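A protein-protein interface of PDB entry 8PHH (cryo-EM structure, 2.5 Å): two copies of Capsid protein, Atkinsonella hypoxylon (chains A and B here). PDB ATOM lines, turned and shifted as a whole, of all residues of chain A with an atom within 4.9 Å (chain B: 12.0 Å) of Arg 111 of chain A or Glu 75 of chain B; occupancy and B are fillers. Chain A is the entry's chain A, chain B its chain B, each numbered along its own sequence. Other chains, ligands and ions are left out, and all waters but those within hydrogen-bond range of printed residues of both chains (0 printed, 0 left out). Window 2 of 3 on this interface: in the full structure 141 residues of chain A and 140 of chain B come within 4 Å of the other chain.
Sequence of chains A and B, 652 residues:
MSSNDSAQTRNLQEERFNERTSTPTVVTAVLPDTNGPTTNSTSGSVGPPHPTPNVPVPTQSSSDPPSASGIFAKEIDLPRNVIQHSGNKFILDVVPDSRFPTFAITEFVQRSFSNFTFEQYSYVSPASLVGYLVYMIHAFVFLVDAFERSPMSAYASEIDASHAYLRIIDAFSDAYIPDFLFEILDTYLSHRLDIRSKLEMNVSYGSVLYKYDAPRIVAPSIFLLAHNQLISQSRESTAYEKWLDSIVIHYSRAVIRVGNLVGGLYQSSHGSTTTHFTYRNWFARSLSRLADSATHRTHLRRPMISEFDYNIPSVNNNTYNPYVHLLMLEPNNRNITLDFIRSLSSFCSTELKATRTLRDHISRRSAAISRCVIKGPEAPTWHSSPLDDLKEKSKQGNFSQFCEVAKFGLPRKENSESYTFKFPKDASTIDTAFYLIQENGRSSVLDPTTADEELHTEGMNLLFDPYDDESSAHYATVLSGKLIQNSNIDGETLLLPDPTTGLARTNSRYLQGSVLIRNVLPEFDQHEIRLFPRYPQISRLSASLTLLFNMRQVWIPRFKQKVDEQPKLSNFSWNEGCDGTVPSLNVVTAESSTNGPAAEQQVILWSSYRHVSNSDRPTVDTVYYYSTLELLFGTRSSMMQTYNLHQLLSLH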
ATOM      1  N   GLU A 107      25.191 -18.911  -3.448  1.00  0.00           N
ATOM      2  CA  GLU A 107      23.985 -18.131  -3.692  1.00  0.00           C
ATOM      3  C   GLU A 107      23.739 -17.895  -5.182  1.00  0.00           C
ATOM      4  O   GLU A 107      22.581 -17.791  -5.598  1.00  0.00           O
ATOM      5  CB  GLU A 107      24.056 -16.814  -2.919  1.00  0.00           C
ATOM      6  CG  GLU A 107      22.772 -16.004  -2.941  1.00  0.00           C
ATOM      7  CD  GLU A 107      21.606 -16.720  -2.278  1.00  0.00           C
ATOM      8  OE1 GLU A 107      21.827 -17.510  -1.339  1.00  0.00           O
ATOM      9  OE2 GLU A 107      20.457 -16.494  -2.702  1.00  0.00           O
ATOM     10  N   PHE A 108      24.796 -17.842  -5.991  1.00  0.00           N
ATOM     11  CA  PHE A 108      24.669 -17.839  -7.445  1.00  0.00           C
ATOM     12  C   PHE A 108      23.999 -19.099  -7.974  1.00  0.00           C
ATOM     13  O   PHE A 108      23.148 -19.017  -8.865  1.00  0.00           O
ATOM     14  CB  PHE A 108      26.057 -17.684  -8.067  1.00  0.00           C
ATOM     15  CG  PHE A 108      26.089 -17.850  -9.554  1.00  0.00           C
ATOM     16  CD1 PHE A 108      25.635 -16.853 -10.379  1.00  0.00           C
ATOM     17  CD2 PHE A 108      26.603 -19.003 -10.124  1.00  0.00           C
ATOM     18  CE1 PHE A 108      25.675 -16.994 -11.743  1.00  0.00           C
ATOM     19  CE2 PHE A 108      26.639 -19.155 -11.488  1.00  0.00           C
ATOM     20  CZ  PHE A 108      26.175 -18.149 -12.296  1.00  0.00           C
ATOM     21  N   VAL A 109      24.379 -20.261  -7.447  1.00  0.00           N
ATOM     22  CA  VAL A 109      23.827 -21.523  -7.931  1.00  0.00           C
ATOM     23  C   VAL A 109      22.396 -21.697  -7.436  1.00  0.00           C
ATOM     24  O   VAL A 109      21.547 -22.269  -8.130  1.00  0.00           O
ATOM     25  CB  VAL A 109      24.754 -22.685  -7.520  1.00  0.00           C
ATOM     26  CG1 VAL A 109      24.162 -24.045  -7.812  1.00  0.00           C
ATOM     27  CG2 VAL A 109      26.055 -22.557  -8.270  1.00  0.00           C
ATOM     28  N   GLN A 110      22.092 -21.144  -6.256  1.00  0.00           N
ATOM     29  CA  GLN A 110      20.728 -21.174  -5.729  1.00  0.00           C
ATOM     30  C   GLN A 110      19.744 -20.443  -6.634  1.00  0.00           C
ATOM     31  O   GLN A 110      18.622 -20.911  -6.851  1.00  0.00           O
ATOM     32  CB  GLN A 110      20.703 -20.570  -4.328  1.00  0.00           C
ATOM     33  CG  GLN A 110      19.320 -20.465  -3.717  1.00  0.00           C
ATOM     34  CD  GLN A 110      18.687 -21.801  -3.436  1.00  0.00           C
ATOM     35  OE1 GLN A 110      19.336 -22.717  -2.932  1.00  0.00           O
ATOM     36  NE2 GLN A 110      17.416 -21.930  -3.772  1.00  0.00           N
ATOM     37  N   ARG A 111      20.158 -19.331  -7.214  1.00  0.00           N
ATOM     38  CA  ARG A 111      19.247 -18.499  -7.976  1.00  0.00           C
ATOM     39  C   ARG A 111      19.233 -18.822  -9.457  1.00  0.00           C
ATOM     40  O   ARG A 111      18.525 -18.153 -10.212  1.00  0.00           O
ATOM     41  CB  ARG A 111      19.604 -17.035  -7.768  1.00  0.00           C
ATOM     42  CG  ARG A 111      19.543 -16.675  -6.326  1.00  0.00           C
ATOM     43  CD  ARG A 111      19.747 -15.223  -6.094  1.00  0.00           C
ATOM     44  NE  ARG A 111      19.837 -14.974  -4.670  1.00  0.00           N
ATOM     45  CZ  ARG A 111      19.883 -13.768  -4.136  1.00  0.00           C
ATOM     46  NH1 ARG A 111      19.809 -12.703  -4.914  1.00  0.00           N
ATOM     47  NH2 ARG A 111      19.963 -13.638  -2.823  1.00  0.00           N
ATOM     48  N   SER A 112      19.983 -19.828  -9.896  1.00  0.00           N
ATOM     49  CA  SER A 112      20.107 -20.049 -11.329  1.00  0.00           C
ATOM     50  C   SER A 112      20.007 -21.509 -11.747  1.00  0.00           C
ATOM     51  O   SER A 112      19.936 -21.787 -12.946  1.00  0.00           O
ATOM     52  CB  SER A 112      21.428 -19.463 -11.826  1.00  0.00           C
ATOM     53  OG  SER A 112      22.530 -20.151 -11.264  1.00  0.00           O
ATOM     54  N   PHE A 113      19.994 -22.448 -10.798  1.00  0.00           N
ATOM     55  CA  PHE A 113      20.140 -23.848 -11.185  1.00  0.00           C
ATOM     56  C   PHE A 113      18.879 -24.422 -11.811  1.00  0.00           C
ATOM     57  O   PHE A 113      18.973 -25.348 -12.622  1.00  0.00           O
ATOM     58  CB  PHE A 113      20.554 -24.715 -10.000  1.00  0.00           C
ATOM     59  CG  PHE A 113      20.948 -26.106 -10.390  1.00  0.00           C
ATOM     60  CD1 PHE A 113      22.170 -26.343 -10.991  1.00  0.00           C
ATOM     61  CD2 PHE A 113      20.087 -27.171 -10.188  1.00  0.00           C
ATOM     62  CE1 PHE A 113      22.534 -27.612 -11.369  1.00  0.00           C
ATOM     63  CE2 PHE A 113      20.448 -28.443 -10.566  1.00  0.00           C
ATOM     64  CZ  PHE A 113      21.674 -28.661 -11.159  1.00  0.00           C
ATOM     65  N   ASN A 115      17.075 -23.165 -14.054  1.00  0.00           N
ATOM     66  CA  ASN A 115      17.019 -22.831 -15.466  1.00  0.00           C
ATOM     67  C   ASN A 115      17.895 -23.733 -16.319  1.00  0.00           C
ATOM     68  O   ASN A 115      18.061 -23.461 -17.510  1.00  0.00           O
ATOM     69  CB  ASN A 115      17.439 -21.378 -15.674  1.00  0.00           C
ATOM     70  CG  ASN A 115      16.468 -20.404 -15.062  1.00  0.00           C
ATOM     71  OD1 ASN A 115      15.256 -20.574 -15.160  1.00  0.00           O
ATOM     72  ND2 ASN A 115      16.994 -19.372 -14.423  1.00  0.00           N
ATOM     73  N   LEU A 648      24.615  -8.851   4.042  1.00  0.00           N
ATOM     74  CA  LEU A 648      24.458  -8.117   2.796  1.00  0.00           C
ATOM     75  C   LEU A 648      23.901  -8.974   1.674  1.00  0.00           C
ATOM     76  O   LEU A 648      23.251  -8.453   0.767  1.00  0.00           O
ATOM     77  CB  LEU A 648      25.801  -7.539   2.356  1.00  0.00           C
ATOM     78  CG  LEU A 648      26.432  -6.375   3.112  1.00  0.00           C
ATOM     79  CD1 LEU A 648      27.845  -6.159   2.624  1.00  0.00           C
ATOM     80  CD2 LEU A 648      25.616  -5.117   2.944  1.00  0.00           C
ATOM     81  N   LEU A 649      24.161 -10.272   1.709  1.00  0.00           N
ATOM     82  CA  LEU A 649      23.749 -11.204   0.673  1.00  0.00           C
ATOM     83  C   LEU A 649      22.856 -12.243   1.334  1.00  0.00           C
ATOM     84  O   LEU A 649      23.337 -13.092   2.091  1.00  0.00           O
ATOM     85  CB  LEU A 649      24.968 -11.845   0.020  1.00  0.00           C
ATOM     86  CG  LEU A 649      24.768 -12.709  -1.214  1.00  0.00           C
ATOM     87  CD1 LEU A 649      24.283 -11.853  -2.339  1.00  0.00           C
ATOM     88  CD2 LEU A 649      26.064 -13.382  -1.578  1.00  0.00           C
ATOM     89  N   SER A 650      21.561 -12.171   1.060  1.00  0.00           N
ATOM     90  CA  SER A 650      20.590 -13.041   1.699  1.00  0.00           C
ATOM     91  C   SER A 650      20.614 -14.431   1.083  1.00  0.00           C
ATOM     92  O   SER A 650      21.117 -14.633  -0.022  1.00  0.00           O
ATOM     93  CB  SER A 650      19.186 -12.454   1.582  1.00  0.00           C
ATOM     94  OG  SER A 650      18.764 -12.433   0.232  1.00  0.00           O
ATOM     95  N   HIS A 652      18.268 -16.972  -0.396  1.00  0.00           N
ATOM     96  CA  HIS A 652      16.985 -17.428  -0.916  1.00  0.00           C
ATOM     97  C   HIS A 652      17.131 -18.102  -2.274  1.00  0.00           C
ATOM     98  O   HIS A 652      17.814 -17.601  -3.168  1.00  0.00           O
ATOM     99  CB  HIS A 652      15.976 -16.276  -1.006  1.00  0.00           C
ATOM    100  CG  HIS A 652      16.331 -15.208  -1.996  1.00  0.00           C
ATOM    101  ND1 HIS A 652      16.071 -15.329  -3.344  1.00  0.00           N
ATOM    102  CD2 HIS A 652      16.858 -13.973  -1.824  1.00  0.00           C
ATOM    103  CE1 HIS A 652      16.458 -14.230  -3.963  1.00  0.00           C
ATOM    104  NE2 HIS A 652      16.934 -13.390  -3.063  1.00  0.00           N
ATOM    105  N   SER B  69      25.949  -4.644 -13.686  1.00  0.00           N
ATOM    106  CA  SER B  69      27.305  -4.417 -13.132  1.00  0.00           C
ATOM    107  C   SER B  69      27.543  -5.354 -11.953  1.00  0.00           C
ATOM    108  O   SER B  69      28.050  -4.887 -10.936  1.00  0.00           O
ATOM    109  CB  SER B  69      27.475  -2.995 -12.714  1.00  0.00           C
ATOM    110  OG  SER B  69      28.405  -2.888 -11.648  1.00  0.00           O
ATOM    111  N   GLY B  70      27.282  -6.632 -12.150  1.00  0.00           N
ATOM    112  CA  GLY B  70      27.472  -7.596 -11.069  1.00  0.00           C
ATOM    113  C   GLY B  70      26.168  -8.285 -10.831  1.00  0.00           C
ATOM    114  O   GLY B  70      25.165  -7.614 -10.807  1.00  0.00           O
ATOM    115  N   ILE B  71      26.196  -9.585 -10.633  1.00  0.00           N
ATOM    116  CA  ILE B  71      24.956 -10.357 -10.404  1.00  0.00           C
ATOM    117  C   ILE B  71      24.292  -9.867  -9.126  1.00  0.00           C
ATOM    118  O   ILE B  71      23.082  -9.688  -9.133  1.00  0.00           O
ATOM    119  CB  ILE B  71      25.266 -11.857 -10.360  1.00  0.00           C
ATOM    120  CG1 ILE B  71      26.488 -12.166  -9.496  1.00  0.00           C
ATOM    121  CG2 ILE B  71      25.439 -12.376 -11.759  1.00  0.00           C
ATOM    122  CD1 ILE B  71      26.503 -13.568  -8.936  1.00  0.00           C
ATOM    123  N   PHE B  72      25.074  -9.598  -8.100  1.00  0.00           N
ATOM    124  CA  PHE B  72      24.540  -9.214  -6.787  1.00  0.00           C
ATOM    125  C   PHE B  72      24.695  -7.734  -6.485  1.00  0.00           C
ATOM    126  O   PHE B  72      24.499  -7.392  -5.347  1.00  0.00           O
ATOM    127  CB  PHE B  72      25.325 -10.011  -5.767  1.00  0.00           C
ATOM    128  CG  PHE B  72      25.097 -11.483  -5.872  1.00  0.00           C
ATOM    129  CD1 PHE B  72      23.874 -11.972  -6.263  1.00  0.00           C
ATOM    130  CD2 PHE B  72      26.068 -12.374  -5.495  1.00  0.00           C
ATOM    131  CE1 PHE B  72      23.642 -13.328  -6.323  1.00  0.00           C
ATOM    132  CE2 PHE B  72      25.830 -13.729  -5.553  1.00  0.00           C
ATOM    133  CZ  PHE B  72      24.616 -14.201  -5.953  1.00  0.00           C
ATOM    134  N   ALA B  73      24.963  -6.890  -7.468  1.00  0.00           N
ATOM    135  CA  ALA B  73      25.165  -5.479  -7.167  1.00  0.00           C
ATOM    136  C   ALA B  73      23.868  -4.812  -6.736  1.00  0.00           C
ATOM    137  O   ALA B  73      23.875  -3.938  -5.867  1.00  0.00           O
ATOM    138  CB  ALA B  73      25.759  -4.762  -8.374  1.00  0.00           C
ATOM    139  N   LYS B  74      22.746  -5.200  -7.338  1.00  0.00           N
ATOM    140  CA  LYS B  74      21.473  -4.616  -6.935  1.00  0.00           C
ATOM    141  C   LYS B  74      21.000  -5.171  -5.603  1.00  0.00           C
ATOM    142  O   LYS B  74      20.282  -4.485  -4.868  1.00  0.00           O
ATOM    143  CB  LYS B  74      20.409  -4.853  -8.004  1.00  0.00           C
ATOM    144  CG  LYS B  74      20.630  -4.073  -9.280  1.00  0.00           C
ATOM    145  CD  LYS B  74      19.515  -4.337 -10.279  1.00  0.00           C
ATOM    146  CE  LYS B  74      19.740  -3.578 -11.576  1.00  0.00           C
ATOM    147  NZ  LYS B  74      18.650  -3.834 -12.559  1.00  0.00           N
ATOM    148  N   GLU B  75      21.383  -6.400  -5.277  1.00  0.00           N
ATOM    149  CA  GLU B  75      20.955  -6.999  -4.023  1.00  0.00           C
ATOM    150  C   GLU B  75      21.736  -6.455  -2.841  1.00  0.00           C
ATOM    151  O   GLU B  75      21.140  -6.038  -1.841  1.00  0.00           O
ATOM    152  CB  GLU B  75      21.118  -8.508  -4.072  1.00  0.00           C
ATOM    153  CG  GLU B  75      20.709  -9.159  -2.784  1.00  0.00           C
ATOM    154  CD  GLU B  75      20.939 -10.632  -2.802  1.00  0.00           C
ATOM    155  OE1 GLU B  75      21.440 -11.129  -3.831  1.00  0.00           O
ATOM    156  OE2 GLU B  75      20.621 -11.300  -1.797  1.00  0.00           O
ATOM    157  N   ILE B  76      23.064  -6.488  -2.929  1.00  0.00           N
ATOM    158  CA  ILE B  76      23.893  -5.986  -1.841  1.00  0.00           C
ATOM    159  C   ILE B  76      23.743  -4.479  -1.722  1.00  0.00           C
ATOM    160  O   ILE B  76      23.385  -3.958  -0.659  1.00  0.00           O
ATOM    161  CB  ILE B  76      25.360  -6.394  -2.053  1.00  0.00           C
ATOM    162  CG1 ILE B  76      25.493  -7.911  -2.124  1.00  0.00           C
ATOM    163  CG2 ILE B  76      26.180  -5.931  -0.902  1.00  0.00           C
ATOM    164  CD1 ILE B  76      26.864  -8.377  -2.524  1.00  0.00           C
ATOM    165  N   ASP B  77      23.995  -3.773  -2.824  1.00  0.00           N
ATOM    166  CA  ASP B  77      23.799  -2.334  -3.003  1.00  0.00           C
ATOM    167  C   ASP B  77      24.592  -1.540  -1.965  1.00  0.00           C
ATOM    168  O   ASP B  77      24.043  -0.923  -1.056  1.00  0.00           O
ATOM    169  CB  ASP B  77      22.311  -1.973  -2.982  1.00  0.00           C
ATOM    170  CG  ASP B  77      22.020  -0.679  -3.716  1.00  0.00           C
ATOM    171  OD1 ASP B  77      22.034  -0.702  -4.967  1.00  0.00           O
ATOM    172  OD2 ASP B  77      21.788   0.356  -3.077  1.00  0.00           O
ATOM    173  N   LEU B  78      25.915  -1.636  -2.112  1.00  0.00           N
ATOM    174  CA  LEU B  78      26.905  -0.945  -1.290  1.00  0.00           C
ATOM    175  C   LEU B  78      26.678   0.558  -1.112  1.00  0.00           C
ATOM    176  O   LEU B  78      26.905   1.037   0.002  1.00  0.00           O
ATOM    177  CB  LEU B  78      28.327  -1.152  -1.828  1.00  0.00           C
ATOM    178  CG  LEU B  78      29.170  -2.385  -1.514  1.00  0.00           C
ATOM    179  CD1 LEU B  78      29.330  -2.616  -0.027  1.00  0.00           C
ATOM    180  CD2 LEU B  78      28.629  -3.599  -2.203  1.00  0.00           C
ATOM    181  N   PRO B  79      26.241   1.370  -2.145  1.00  0.00           N
ATOM    182  CA  PRO B  79      26.009   2.795  -1.860  1.00  0.00           C
ATOM    183  C   PRO B  79      24.909   3.128  -0.861  1.00  0.00           C
ATOM    184  O   PRO B  79      24.809   4.288  -0.453  1.00  0.00           O
ATOM    185  CB  PRO B  79      25.676   3.373  -3.237  1.00  0.00           C
ATOM    186  CG  PRO B  79      26.366   2.512  -4.166  1.00  0.00           C
ATOM    187  CD  PRO B  79      26.238   1.155  -3.608  1.00  0.00           C
ATOM    188  N   ARG B  80      24.088   2.167  -0.445  1.00  0.00           N
ATOM    189  CA  ARG B  80      23.168   2.409   0.652  1.00  0.00           C
ATOM    190  C   ARG B  80      23.486   1.612   1.906  1.00  0.00           C
ATOM    191  O   ARG B  80      22.732   1.707   2.879  1.00  0.00           O
ATOM    192  CB  ARG B  80      21.718   2.118   0.235  1.00  0.00           C
ATOM    193  CG  ARG B  80      21.346   0.652   0.113  1.00  0.00           C
ATOM    194  CD  ARG B  80      19.909   0.513  -0.380  1.00  0.00           C
ATOM    195  NE  ARG B  80      19.765   1.009  -1.747  1.00  0.00           N
ATOM    196  CZ  ARG B  80      18.601   1.175  -2.366  1.00  0.00           C
ATOM    197  NH1 ARG B  80      17.469   0.885  -1.742  1.00  0.00           N
ATOM    198  NH2 ARG B  80      18.568   1.635  -3.610  1.00  0.00           N
ATOM    199  N   ASN B  81      24.580   0.855   1.926  1.00  0.00           N
ATOM    200  CA  ASN B  81      24.925   0.018   3.064  1.00  0.00           C
ATOM    201  C   ASN B  81      26.353   0.239   3.547  1.00  0.00           C
ATOM    202  O   ASN B  81      26.857  -0.545   4.355  1.00  0.00           O
ATOM    203  CB  ASN B  81      24.698  -1.449   2.719  1.00  0.00           C
ATOM    204  CG  ASN B  81      23.238  -1.806   2.660  1.00  0.00           C
ATOM    205  OD1 ASN B  81      22.461  -1.420   3.526  1.00  0.00           O
ATOM    206  ND2 ASN B  81      22.851  -2.536   1.628  1.00  0.00           N
ATOM    207  N   VAL B  82      27.017   1.287   3.070  1.00  0.00           N
ATOM    208  CA  VAL B  82      28.307   1.698   3.606  1.00  0.00           C
ATOM    209  C   VAL B  82      28.112   2.976   4.402  1.00  0.00           C
ATOM    210  O   VAL B  82      27.166   3.733   4.166  1.00  0.00           O
ATOM    211  CB  VAL B  82      29.389   1.903   2.521  1.00  0.00           C
ATOM    212  CG1 VAL B  82      29.671   0.614   1.796  1.00  0.00           C
ATOM    213  CG2 VAL B  82      29.009   3.003   1.555  1.00  0.00           C
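The guanidinium group (NH1) of Arg 111 of chain A lies within salt-bridge range of the side-chain carboxylate (OE1) of Glu 75 of chain B (2.5 Å). The side-chain carboxylate of Glu 75 of chain B lies within hydrogen-bond range of the side-chain hydroxyl of Ser 650 of chain A (3.0 Å).
Of the printed residues of chain B, Glu 107 of chain A touches Phe 72. Phe 108 of chain A touches two residues of chain B. No residue of chain B comes within 4 Å of Val 109 of chain A. No residue of chain B comes within 4 Å of Ser 112 of chain A. Printed residues of chain B within 4 Å of Leu 648 of chain A: Ile 76 (3.6 Å) and Asn 81 (3.8 Å). Leu 649 of chain A touches just these residues of chain B: Phe 72 and Glu 75. Ser 650 of chain A touches just one residue of chain B: Glu 75 (3.0 Å). No residue of chain B comes within 4 Å of His 652 of chain A. Of chain A, only Arg 111 (2.5 Å), Leu 649 (3.3 Å) and Ser 650 (3.0 Å) come within 4 Å of Glu 75 of chain B. Of the printed residues of chain A, Ile 76 of chain B touches Leu 648 (3.6 Å). Leu 78 of chain B touches none of the printed residues of chain A. Pro 79 of chain B touches none of the printed residues of chain A. Printed residues of chain A within 4 Å of Asn 81 of chain B: Leu 648. The nearest residue of chain A that does not touch Glu 75 of chain B is Leu 648 of chain A (4.1 Å). The nearest printed residue of chain A that does not touch Phe 72 of chain B is Arg 111 of chain A (4.1 Å).
No position is printed for both chains. Of the 9 pairs that touch across the chains among the printed residues, none has its exchanged pair printed and touching as well.
Hydrophobic or aromatic side chains of chain B within 4 Å of the printed part of chain A: Ile 71, Phe 72 and Ile 76. Of the 12 printed residues of chain A, 6 touch a printed residue of chain B. Printed residues of chain A that touch a printed residue of chain B: Glu 107, Phe 108, Arg 111, Leu 648, Leu 649 and Ser 650. Hydrophobic or aromatic side chains of chain A that line the printed part of chain B: Phe 108, Leu 648 and Leu 649.
The side-chain carboxylate (OE2) of Glu 107 of chain A sits at hydrogen-bond distance from the backbone NH (N) of His 652 of chain A. The side-chain carboxylate (OE2) of Glu 107 of chain A lies within salt-bridge range of the guanidinium group (NE) of Arg 111 of chain A (2.6 Å). NE2 of His 652 of chain A lies within hydrogen-bond range of NH2 of Arg 111 of chain A. O of Asp 77 of chain B is in hydrogen-bond range of ND2 of Asn 81 of chain B (3.4 Å). OG of Ser 112 of chain A is in hydrogen-bond range of O of Phe 108 of chain A. NH2 of Arg 111 of chain A sits at hydrogen-bond distance from O of Ser 650 of chain A (3.2 Å).
Among the printed residues, pairs that only touch across the chains: Glu 107 of chain A with Phe 72 of chain B (3.9 Å), Phe 108 of chain A with Ile 71 of chain B (3.7 Å), Phe 108 of chain A with Phe 72 of chain B (3.6 Å), Leu 648 of chain A with Ile 76 of chain B (3.6 Å), Leu 648 of chain A with Asn 81 of chain B (3.8 Å), Leu 649 of chain A with Phe 72 of chain B (3.6 Å) and Leu 649 of chain A with Glu 75 of chain B (3.3 Å).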
